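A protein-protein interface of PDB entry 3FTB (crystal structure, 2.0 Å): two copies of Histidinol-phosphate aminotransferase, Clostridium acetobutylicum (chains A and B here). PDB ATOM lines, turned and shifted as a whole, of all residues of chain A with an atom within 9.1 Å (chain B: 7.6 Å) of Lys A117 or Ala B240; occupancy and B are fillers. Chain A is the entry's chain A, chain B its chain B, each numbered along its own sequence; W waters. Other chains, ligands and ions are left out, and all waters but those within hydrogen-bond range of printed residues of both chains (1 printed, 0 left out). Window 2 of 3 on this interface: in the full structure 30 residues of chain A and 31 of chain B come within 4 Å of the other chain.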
ATOM      1  N   SER A  88      21.884 -27.045  27.668  1.00  0.00           N
ATOM      2  CA  SER A  88      21.834 -26.767  26.238  1.00  0.00           C
ATOM      3  C   SER A  88      20.622 -27.395  25.581  1.00  0.00           C
ATOM      4  O   SER A  88      19.959 -26.774  24.755  1.00  0.00           O
ATOM      5  CB  SER A  88      23.089 -27.303  25.554  1.00  0.00           C
ATOM      6  OG  SER A  88      24.253 -26.903  26.245  1.00  0.00           O
ATOM      7  N   GLU A  89      20.352 -28.642  25.941  1.00  0.00           N
ATOM      8  CA  GLU A  89      19.303 -29.407  25.287  1.00  0.00           C
ATOM      9  C   GLU A  89      17.950 -28.745  25.538  1.00  0.00           C
ATOM     10  O   GLU A  89      17.080 -28.710  24.664  1.00  0.00           O
ATOM     11  CB  GLU A  89      19.316 -30.867  25.780  1.00  0.00           C
ATOM     12  CG  GLU A  89      18.599 -31.869  24.860  1.00  0.00           C
ATOM     13  CD  GLU A  89      18.507 -33.300  25.430  1.00  0.00           C
ATOM     14  OE1 GLU A  89      19.213 -33.612  26.409  1.00  0.00           O
ATOM     15  OE2 GLU A  89      17.727 -34.124  24.893  1.00  0.00           O
ATOM     16  N   ILE A  91      17.277 -25.455  26.483  1.00  0.00           N
ATOM     17  CA  ILE A  91      17.190 -24.159  25.812  1.00  0.00           C
ATOM     18  C   ILE A  91      16.736 -24.337  24.364  1.00  0.00           C
ATOM     19  O   ILE A  91      15.739 -23.745  23.933  1.00  0.00           O
ATOM     20  CB  ILE A  91      18.550 -23.440  25.826  1.00  0.00           C
ATOM     21  CG1 ILE A  91      18.969 -23.131  27.269  1.00  0.00           C
ATOM     22  CG2 ILE A  91      18.496 -22.172  24.977  1.00  0.00           C
ATOM     23  CD1 ILE A  91      20.366 -22.566  27.394  1.00  0.00           C
ATOM     24  N   GLU A  92      17.462 -25.168  23.621  1.00  0.00           N
ATOM     25  CA  GLU A  92      17.081 -25.484  22.249  1.00  0.00           C
ATOM     26  C   GLU A  92      15.653 -26.018  22.155  1.00  0.00           C
ATOM     27  O   GLU A  92      14.842 -25.490  21.396  1.00  0.00           O
ATOM     28  CB  GLU A  92      18.049 -26.493  21.624  1.00  0.00           C
ATOM     29  CG  GLU A  92      17.535 -27.102  20.326  1.00  0.00           C
ATOM     30  CD  GLU A  92      18.607 -27.862  19.574  1.00  0.00           C
ATOM     31  OE1 GLU A  92      19.773 -27.421  19.601  1.00  0.00           O
ATOM     32  OE2 GLU A  92      18.284 -28.898  18.953  1.00  0.00           O
ATOM     33  N   LEU A  93      15.356 -27.062  22.932  1.00  0.00           N
ATOM     34  CA  LEU A  93      14.072 -27.760  22.847  1.00  0.00           C
ATOM     35  C   LEU A  93      12.874 -26.901  23.220  1.00  0.00           C
ATOM     36  O   LEU A  93      11.838 -26.949  22.554  1.00  0.00           O
ATOM     37  CB  LEU A  93      14.074 -29.022  23.710  1.00  0.00           C
ATOM     38  CG  LEU A  93      14.814 -30.222  23.126  1.00  0.00           C
ATOM     39  CD1 LEU A  93      14.965 -31.269  24.186  1.00  0.00           C
ATOM     40  CD2 LEU A  93      14.091 -30.779  21.912  1.00  0.00           C
ATOM     41  N   ILE A  95      12.708 -23.764  22.966  1.00  0.00           N
ATOM     42  CA  ILE A  95      12.567 -22.758  21.921  1.00  0.00           C
ATOM     43  C   ILE A  95      12.068 -23.408  20.625  1.00  0.00           C
ATOM     44  O   ILE A  95      11.420 -22.755  19.796  1.00  0.00           O
ATOM     45  CB  ILE A  95      13.895 -21.991  21.695  1.00  0.00           C
ATOM     46  CG1 ILE A  95      14.217 -21.106  22.905  1.00  0.00           C
ATOM     47  CG2 ILE A  95      13.840 -21.153  20.417  1.00  0.00           C
ATOM     48  CD1 ILE A  95      15.623 -20.513  22.870  1.00  0.00           C
ATOM     49  N   SER A  96      12.345 -24.701  20.470  1.00  0.00           N
ATOM     50  CA  SER A  96      11.911 -25.453  19.292  1.00  0.00           C
ATOM     51  C   SER A  96      10.394 -25.544  19.197  1.00  0.00           C
ATOM     52  O   SER A  96       9.854 -25.903  18.149  1.00  0.00           O
ATOM     53  CB  SER A  96      12.510 -26.865  19.291  1.00  0.00           C
ATOM     54  OG  SER A  96      11.814 -27.738  20.174  1.00  0.00           O
ATOM     55  N   PHE A  98       8.090 -23.090  19.620  1.00  0.00           N
ATOM     56  CA  PHE A  98       7.348 -21.903  19.193  1.00  0.00           C
ATOM     57  C   PHE A  98       7.764 -21.399  17.824  1.00  0.00           C
ATOM     58  O   PHE A  98       8.831 -21.748  17.326  1.00  0.00           O
ATOM     59  CB  PHE A  98       7.479 -20.798  20.234  1.00  0.00           C
ATOM     60  CG  PHE A  98       7.319 -21.293  21.626  1.00  0.00           C
ATOM     61  CD1 PHE A  98       6.068 -21.610  22.112  1.00  0.00           C
ATOM     62  CD2 PHE A  98       8.423 -21.492  22.437  1.00  0.00           C
ATOM     63  CE1 PHE A  98       5.914 -22.090  23.399  1.00  0.00           C
ATOM     64  CE2 PHE A  98       8.279 -21.968  23.717  1.00  0.00           C
ATOM     65  CZ  PHE A  98       7.021 -22.276  24.203  1.00  0.00           C
ATOM     66  N   GLU A 110      23.272 -18.598  22.592  1.00  0.00           N
ATOM     67  CA  GLU A 110      22.459 -19.784  22.291  1.00  0.00           C
ATOM     68  C   GLU A 110      20.938 -19.555  22.143  1.00  0.00           C
ATOM     69  O   GLU A 110      20.256 -20.344  21.483  1.00  0.00           O
ATOM     70  CB  GLU A 110      22.737 -20.916  23.301  1.00  0.00           C
ATOM     71  CG  GLU A 110      21.592 -21.951  23.389  1.00  0.00           C
ATOM     72  CD  GLU A 110      21.987 -23.297  24.015  1.00  0.00           C
ATOM     73  OE1 GLU A 110      22.552 -23.302  25.129  1.00  0.00           O
ATOM     74  OE2 GLU A 110      21.704 -24.355  23.400  1.00  0.00           O
ATOM     75  N   TYR A 111      20.389 -18.501  22.742  1.00  0.00           N
ATOM     76  CA  TYR A 111      18.956 -18.275  22.565  1.00  0.00           C
ATOM     77  C   TYR A 111      18.630 -18.108  21.073  1.00  0.00           C
ATOM     78  O   TYR A 111      17.797 -18.837  20.540  1.00  0.00           O
ATOM     79  CB  TYR A 111      18.430 -17.083  23.375  1.00  0.00           C
ATOM     80  CG  TYR A 111      18.790 -17.077  24.847  1.00  0.00           C
ATOM     81  CD1 TYR A 111      19.131 -18.251  25.508  1.00  0.00           C
ATOM     82  CD2 TYR A 111      18.766 -15.899  25.580  1.00  0.00           C
ATOM     83  CE1 TYR A 111      19.459 -18.252  26.854  1.00  0.00           C
ATOM     84  CE2 TYR A 111      19.099 -15.888  26.936  1.00  0.00           C
ATOM     85  CZ  TYR A 111      19.444 -17.073  27.564  1.00  0.00           C
ATOM     86  OH  TYR A 111      19.771 -17.076  28.902  1.00  0.00           O
ATOM     87  N   GLU A 112      19.303 -17.163  20.414  1.00  0.00           N
ATOM     88  CA  GLU A 112      19.069 -16.850  18.998  1.00  0.00           C
ATOM     89  C   GLU A 112      19.619 -17.890  18.014  1.00  0.00           C
ATOM     90  O   GLU A 112      19.038 -18.120  16.944  1.00  0.00           O
ATOM     91  CB  GLU A 112      19.656 -15.480  18.647  1.00  0.00           C
ATOM     92  CG  GLU A 112      19.470 -15.101  17.182  1.00  0.00           C
ATOM     93  CD  GLU A 112      20.261 -13.878  16.771  1.00  0.00           C
ATOM     94  OE1 GLU A 112      21.064 -13.384  17.593  1.00  0.00           O
ATOM     95  OE2 GLU A 112      20.080 -13.414  15.623  1.00  0.00           O
ATOM     96  N   ILE A 113      20.754 -18.486  18.359  1.00  0.00           N
ATOM     97  CA  ILE A 113      21.313 -19.568  17.565  1.00  0.00           C
ATOM     98  C   ILE A 113      20.241 -20.630  17.367  1.00  0.00           C
ATOM     99  O   ILE A 113      19.913 -21.001  16.241  1.00  0.00           O
ATOM    100  CB  ILE A 113      22.470 -20.247  18.299  1.00  0.00           C
ATOM    101  CG1 ILE A 113      23.636 -19.280  18.478  1.00  0.00           C
ATOM    102  CG2 ILE A 113      22.901 -21.515  17.558  1.00  0.00           C
ATOM    103  CD1 ILE A 113      24.728 -19.824  19.394  1.00  0.00           C
ATOM    104  N   ASN A 114      19.700 -21.112  18.481  1.00  0.00           N
ATOM    105  CA  ASN A 114      18.711 -22.189  18.460  1.00  0.00           C
ATOM    106  C   ASN A 114      17.420 -21.806  17.766  1.00  0.00           C
ATOM    107  O   ASN A 114      16.853 -22.598  17.018  1.00  0.00           O
ATOM    108  CB  ASN A 114      18.436 -22.694  19.871  1.00  0.00           C
ATOM    109  CG  ASN A 114      19.549 -23.574  20.386  1.00  0.00           C
ATOM    110  OD1 ASN A 114      20.011 -23.414  21.509  1.00  0.00           O
ATOM    111  ND2 ASN A 114      20.003 -24.504  19.553  1.00  0.00           N
ATOM    112  N   ALA A 115      16.961 -20.587  18.018  1.00  0.00           N
ATOM    113  CA  ALA A 115      15.808 -20.049  17.315  1.00  0.00           C
ATOM    114  C   ALA A 115      15.968 -20.229  15.809  1.00  0.00           C
ATOM    115  O   ALA A 115      15.143 -20.887  15.173  1.00  0.00           O
ATOM    116  CB  ALA A 115      15.589 -18.568  17.669  1.00  0.00           C
ATOM    117  N   LYS A 116      17.026 -19.641  15.249  1.00  0.00           N
ATOM    118  CA  LYS A 116      17.347 -19.824  13.832  1.00  0.00           C
ATOM    119  C   LYS A 116      17.430 -21.310  13.481  1.00  0.00           C
ATOM    120  O   LYS A 116      16.936 -21.734  12.440  1.00  0.00           O
ATOM    121  CB  LYS A 116      18.648 -19.097  13.458  1.00  0.00           C
ATOM    122  CG  LYS A 116      18.596 -17.581  13.682  1.00  0.00           C
ATOM    123  CD  LYS A 116      19.532 -16.786  12.746  1.00  0.00           C
ATOM    124  CE  LYS A 116      20.988 -16.895  13.162  1.00  0.00           C
ATOM    125  NZ  LYS A 116      21.770 -15.660  12.856  1.00  0.00           N
ATOM    126  N   LYS A 117      18.036 -22.100  14.366  1.00  0.00           N
ATOM    127  CA  LYS A 117      18.167 -23.545  14.173  1.00  0.00           C
ATOM    128  C   LYS A 117      16.827 -24.264  13.991  1.00  0.00           C
ATOM    129  O   LYS A 117      16.771 -25.364  13.431  1.00  0.00           O
ATOM    130  CB  LYS A 117      18.935 -24.175  15.341  1.00  0.00           C
ATOM    131  CG  LYS A 117      18.986 -25.692  15.295  1.00  0.00           C
ATOM    132  CD  LYS A 117      19.993 -26.278  16.274  1.00  0.00           C
ATOM    133  CE  LYS A 117      19.905 -27.801  16.299  1.00  0.00           C
ATOM    134  NZ  LYS A 117      21.096 -28.433  16.934  1.00  0.00           N
ATOM    135  N   HIS A 118      15.752 -23.651  14.473  1.00  0.00           N
ATOM    136  CA  HIS A 118      14.434 -24.279  14.423  1.00  0.00           C
ATOM    137  C   HIS A 118      13.389 -23.419  13.716  1.00  0.00           C
ATOM    138  O   HIS A 118      12.198 -23.660  13.845  1.00  0.00           O
ATOM    139  CB  HIS A 118      13.962 -24.663  15.831  1.00  0.00           C
ATOM    140  CG  HIS A 118      14.727 -25.805  16.430  1.00  0.00           C
ATOM    141  ND1 HIS A 118      14.414 -27.126  16.179  1.00  0.00           N
ATOM    142  CD2 HIS A 118      15.803 -25.822  17.253  1.00  0.00           C
ATOM    143  CE1 HIS A 118      15.262 -27.907  16.827  1.00  0.00           C
ATOM    144  NE2 HIS A 118      16.115 -27.142  17.484  1.00  0.00           N
ATOM    145  N   GLY A 119      13.840 -22.417  12.970  1.00  0.00           N
ATOM    146  CA  GLY A 119      12.940 -21.564  12.208  1.00  0.00           C
ATOM    147  C   GLY A 119      11.997 -20.676  13.007  1.00  0.00           C
ATOM    148  O   GLY A 119      10.944 -20.272  12.507  1.00  0.00           O
ATOM    149  N   VAL A 120      12.370 -20.360  14.244  1.00  0.00           N
ATOM    150  CA  VAL A 120      11.553 -19.488  15.084  1.00  0.00           C
ATOM    151  C   VAL A 120      11.785 -18.031  14.713  1.00  0.00           C
ATOM    152  O   VAL A 120      12.918 -17.609  14.508  1.00  0.00           O
ATOM    153  CB  VAL A 120      11.882 -19.681  16.573  1.00  0.00           C
ATOM    154  CG1 VAL A 120      10.954 -18.860  17.438  1.00  0.00           C
ATOM    155  CG2 VAL A 120      11.802 -21.162  16.958  1.00  0.00           C
ATOM    156  N   SER A 121      10.707 -17.256  14.629  1.00  0.00           N
ATOM    157  CA  SER A 121      10.812 -15.820  14.377  1.00  0.00           C
ATOM    158  C   SER A 121      11.365 -15.101  15.608  1.00  0.00           C
ATOM    159  O   SER A 121      11.004 -15.424  16.743  1.00  0.00           O
ATOM    160  CB  SER A 121       9.450 -15.239  13.999  1.00  0.00           C
ATOM    161  OG  SER A 121       8.849 -15.999  12.971  1.00  0.00           O
ATOM    162  N   VAL A 122      12.243 -14.131  15.381  1.00  0.00           N
ATOM    163  CA  VAL A 122      12.905 -13.440  16.478  1.00  0.00           C
ATOM    164  C   VAL A 122      12.544 -11.966  16.532  1.00  0.00           C
ATOM    165  O   VAL A 122      12.603 -11.253  15.524  1.00  0.00           O
ATOM    166  CB  VAL A 122      14.439 -13.590  16.395  1.00  0.00           C
ATOM    167  CG1 VAL A 122      15.131 -12.535  17.244  1.00  0.00           C
ATOM    168  CG2 VAL A 122      14.847 -14.979  16.838  1.00  0.00           C
ATOM    169  N   LEU B  93      18.397 -40.084  14.425  1.00  0.00           N
ATOM    170  CA  LEU B  93      18.833 -38.981  13.591  1.00  0.00           C
ATOM    171  C   LEU B  93      19.023 -39.409  12.143  1.00  0.00           C
ATOM    172  O   LEU B  93      18.435 -38.823  11.237  1.00  0.00           O
ATOM    173  CB  LEU B  93      20.085 -38.309  14.171  1.00  0.00           C
ATOM    174  CG  LEU B  93      19.756 -37.249  15.241  1.00  0.00           C
ATOM    175  CD1 LEU B  93      21.002 -36.637  15.847  1.00  0.00           C
ATOM    176  CD2 LEU B  93      18.854 -36.162  14.675  1.00  0.00           C
ATOM    177  N   ILE B 234      26.304 -36.526   4.674  1.00  0.00           N
ATOM    178  CA  ILE B 234      25.444 -37.264   5.575  1.00  0.00           C
ATOM    179  C   ILE B 234      25.931 -37.047   6.991  1.00  0.00           C
ATOM    180  O   ILE B 234      25.136 -36.801   7.900  1.00  0.00           O
ATOM    181  CB  ILE B 234      25.465 -38.763   5.256  1.00  0.00           C
ATOM    182  CG1 ILE B 234      24.451 -39.075   4.162  1.00  0.00           C
ATOM    183  CG2 ILE B 234      25.148 -39.583   6.491  1.00  0.00           C
ATOM    184  CD1 ILE B 234      24.490 -40.522   3.714  1.00  0.00           C
ATOM    185  N   ALA B 235      27.244 -37.131   7.177  1.00  0.00           N
ATOM    186  CA  ALA B 235      27.826 -36.932   8.501  1.00  0.00           C
ATOM    187  C   ALA B 235      27.574 -35.494   9.012  1.00  0.00           C
ATOM    188  O   ALA B 235      27.270 -35.270  10.187  1.00  0.00           O
ATOM    189  CB  ALA B 235      29.323 -37.276   8.473  1.00  0.00           C
ATOM    190  N   ALA B 236      27.671 -34.527   8.106  1.00  0.00           N
ATOM    191  CA  ALA B 236      27.458 -33.125   8.435  1.00  0.00           C
ATOM    192  C   ALA B 236      25.987 -32.850   8.710  1.00  0.00           C
ATOM    193  O   ALA B 236      25.630 -32.266   9.737  1.00  0.00           O
ATOM    194  CB  ALA B 236      27.943 -32.251   7.291  1.00  0.00           C
ATOM    195  N   LYS B 237      25.139 -33.270   7.777  1.00  0.00           N
ATOM    196  CA  LYS B 237      23.722 -32.976   7.848  1.00  0.00           C
ATOM    197  C   LYS B 237      23.140 -33.526   9.141  1.00  0.00           C
ATOM    198  O   LYS B 237      22.165 -33.001   9.674  1.00  0.00           O
ATOM    199  CB  LYS B 237      22.998 -33.557   6.630  1.00  0.00           C
ATOM    200  CG  LYS B 237      21.482 -33.629   6.776  1.00  0.00           C
ATOM    201  CD  LYS B 237      20.760 -33.568   5.431  1.00  0.00           C
ATOM    202  CE  LYS B 237      21.161 -34.704   4.511  1.00  0.00           C
ATOM    203  NZ  LYS B 237      20.236 -34.782   3.341  1.00  0.00           N
ATOM    204  N   ILE B 238      23.760 -34.584   9.646  1.00  0.00           N
ATOM    205  CA  ILE B 238      23.337 -35.203  10.896  1.00  0.00           C
ATOM    206  C   ILE B 238      23.764 -34.413  12.128  1.00  0.00           C
ATOM    207  O   ILE B 238      23.028 -34.341  13.110  1.00  0.00           O
ATOM    208  CB  ILE B 238      23.888 -36.626  11.009  1.00  0.00           C
ATOM    209  CG1 ILE B 238      23.031 -37.584  10.190  1.00  0.00           C
ATOM    210  CG2 ILE B 238      23.923 -37.071  12.461  1.00  0.00           C
ATOM    211  CD1 ILE B 238      23.505 -39.008  10.254  1.00  0.00           C
ATOM    212  N   LYS B 239      24.959 -33.834  12.084  1.00  0.00           N
ATOM    213  CA  LYS B 239      25.478 -33.088  13.223  1.00  0.00           C
ATOM    214  C   LYS B 239      24.811 -31.726  13.330  1.00  0.00           C
ATOM    215  O   LYS B 239      24.731 -31.141  14.409  1.00  0.00           O
ATOM    216  CB  LYS B 239      26.989 -32.935  13.121  1.00  0.00           C
ATOM    217  CG  LYS B 239      27.721 -34.256  12.966  1.00  0.00           C
ATOM    218  CD  LYS B 239      28.988 -34.292  13.809  1.00  0.00           C
ATOM    219  CE  LYS B 239      29.962 -35.349  13.323  1.00  0.00           C
ATOM    220  NZ  LYS B 239      30.563 -34.962  12.012  1.00  0.00           N
ATOM    221  N   ALA B 240      24.316 -31.232  12.205  1.00  0.00           N
ATOM    222  CA  ALA B 240      23.590 -29.976  12.185  1.00  0.00           C
ATOM    223  C   ALA B 240      22.291 -30.098  12.978  1.00  0.00           C
ATOM    224  O   ALA B 240      21.573 -29.115  13.170  1.00  0.00           O
ATOM    225  CB  ALA B 240      23.302 -29.569  10.754  1.00  0.00           C
ATOM    226  N   LYS B 241      21.994 -31.309  13.439  1.00  0.00           N
ATOM    227  CA  LYS B 241      20.771 -31.577  14.188  1.00  0.00           C
ATOM    228  C   LYS B 241      21.054 -31.927  15.651  1.00  0.00           C
ATOM    229  O   LYS B 241      20.128 -32.200  16.427  1.00  0.00           O
ATOM    230  CB  LYS B 241      19.983 -32.713  13.535  1.00  0.00           C
ATOM    231  CG  LYS B 241      19.423 -32.395  12.168  1.00  0.00           C
ATOM    232  CD  LYS B 241      18.431 -33.470  11.771  1.00  0.00           C
ATOM    233  CE  LYS B 241      17.946 -33.271  10.349  1.00  0.00           C
ATOM    234  NZ  LYS B 241      17.288 -34.494   9.829  1.00  0.00           N
ATOM    235  N   GLN B 242      22.334 -31.941  16.013  1.00  0.00           N
ATOM    236  CA  GLN B 242      22.751 -32.310  17.359  1.00  0.00           C
ATOM    237  C   GLN B 242      23.146 -31.057  18.128  1.00  0.00           C
ATOM    238  O   GLN B 242      23.283 -29.981  17.543  1.00  0.00           O
ATOM    239  CB  GLN B 242      23.944 -33.263  17.310  1.00  0.00           C
ATOM    240  CG  GLN B 242      23.818 -34.402  16.296  1.00  0.00           C
ATOM    241  CD  GLN B 242      24.984 -35.378  16.365  1.00  0.00           C
ATOM    242  OE1 GLN B 242      24.908 -36.386  17.056  1.00  0.00           O
ATOM    243  NE2 GLN B 242      26.074 -35.065  15.669  1.00  0.00           N
ATOM    244  N   ASN B 243      23.324 -31.200  19.438  1.00  0.00           N
ATOM    245  CA  ASN B 243      23.863 -30.114  20.254  1.00  0.00           C
ATOM    246  C   ASN B 243      25.373 -30.232  20.461  1.00  0.00           C
ATOM    247  O   ASN B 243      25.933 -31.331  20.448  1.00  0.00           O
ATOM    248  CB  ASN B 243      23.128 -30.012  21.597  1.00  0.00           C
ATOM    249  CG  ASN B 243      21.794 -29.303  21.473  1.00  0.00           C
ATOM    250  OD1 ASN B 243      21.506 -28.351  22.200  1.00  0.00           O
ATOM    251  ND2 ASN B 243      20.982 -29.748  20.524  1.00  0.00           N
ATOM    252  N   PRO B 244      26.045 -29.086  20.616  1.00  0.00           N
ATOM    253  CA  PRO B 244      27.478 -29.091  20.909  1.00  0.00           C
ATOM    254  C   PRO B 244      27.717 -29.703  22.274  1.00  0.00           C
ATOM    255  O   PRO B 244      26.887 -29.531  23.169  1.00  0.00           O
ATOM    256  CB  PRO B 244      27.834 -27.607  20.925  1.00  0.00           C
ATOM    257  CG  PRO B 244      26.755 -26.952  20.118  1.00  0.00           C
ATOM    258  CD  PRO B 244      25.525 -27.727  20.426  1.00  0.00           C
HETATM  259  O   HOH W   1      25.451 -27.470  23.953  1.00  0.00           O
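OE1 of Glu A92 lies within hydrogen-bond range of ND2 of Asn A114 (2.9 Å). The side-chain carboxylate (OE1) of Glu A92 lies within salt-bridge range of the side-chain amino group (NZ) of Lys A117 (3.1 Å). The side-chain carboxylate of Glu A92 is in hydrogen-bond range of a ring nitrogen (NE2) of His A118 (3.2 Å).
Of the printed residues of chain B, Lys A117 touches Ala B240 (3.8 Å), Lys B241 (3.7 Å), Gln B242 (2.7 Å) and Asn B243 (3.8 Å). Of chain A, only Lys A117 comes within 4 Å of Ala B240. Of the printed residues of chain B, Glu A89 touches Asn B243. Of the printed residues of chain A, Asn B243 touches Ser A88 (3.4 Å), Glu A89 (3.9 Å), Glu A92 (2.8 Å) and Lys A117 (3.8 Å). Lys B237 touches none of the printed residues of chain A. The nearest printed residue of chain B that does not touch Ser A88 is Pro B244 (4.8 Å).
Among the printed residues, pairs that only touch across the chains: Lys A117 with Lys B241 (3.7 Å), Lys A117 with Ala B240 (3.8 Å), Lys A117 with Asn B243 (3.8 Å) and Glu A89 with Asn B243 (3.9 Å).
1 position is printed for both chains. Of the 7 pairs that touch across the chains among the printed residues, none has its exchanged pair printed and touching as well.
The backbone carbonyl oxygen of Gln B242 lies within hydrogen-bond range of the side-chain amino group of Lys A117. The side-chain carboxylate of Glu A92 lies within hydrogen-bond range of the side-chain amide nitrogen of Asn B243, 2.8 Å away. OD1 of Asn B243 lies close to O of Ser A88, at 3.4 Å.
Water W1 bridges the backbone carbonyl oxygen (O) of Pro B244 and the side-chain hydroxyl (OG) of Ser A88.
Of the 12 printed residues of chain B, 4 touch a printed residue of chain A. Printed residues of chain B that touch a printed residue of chain A: Ala B240, Lys B241, Gln B242 and Asn B243. Of the 21 printed residues of chain A, 4 touch a printed residue of chain B. Along chain A the printed residues that touch a printed residue of chain B span positions 88 to 117. Among the printed residues, 7 pairs touch across the chains.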
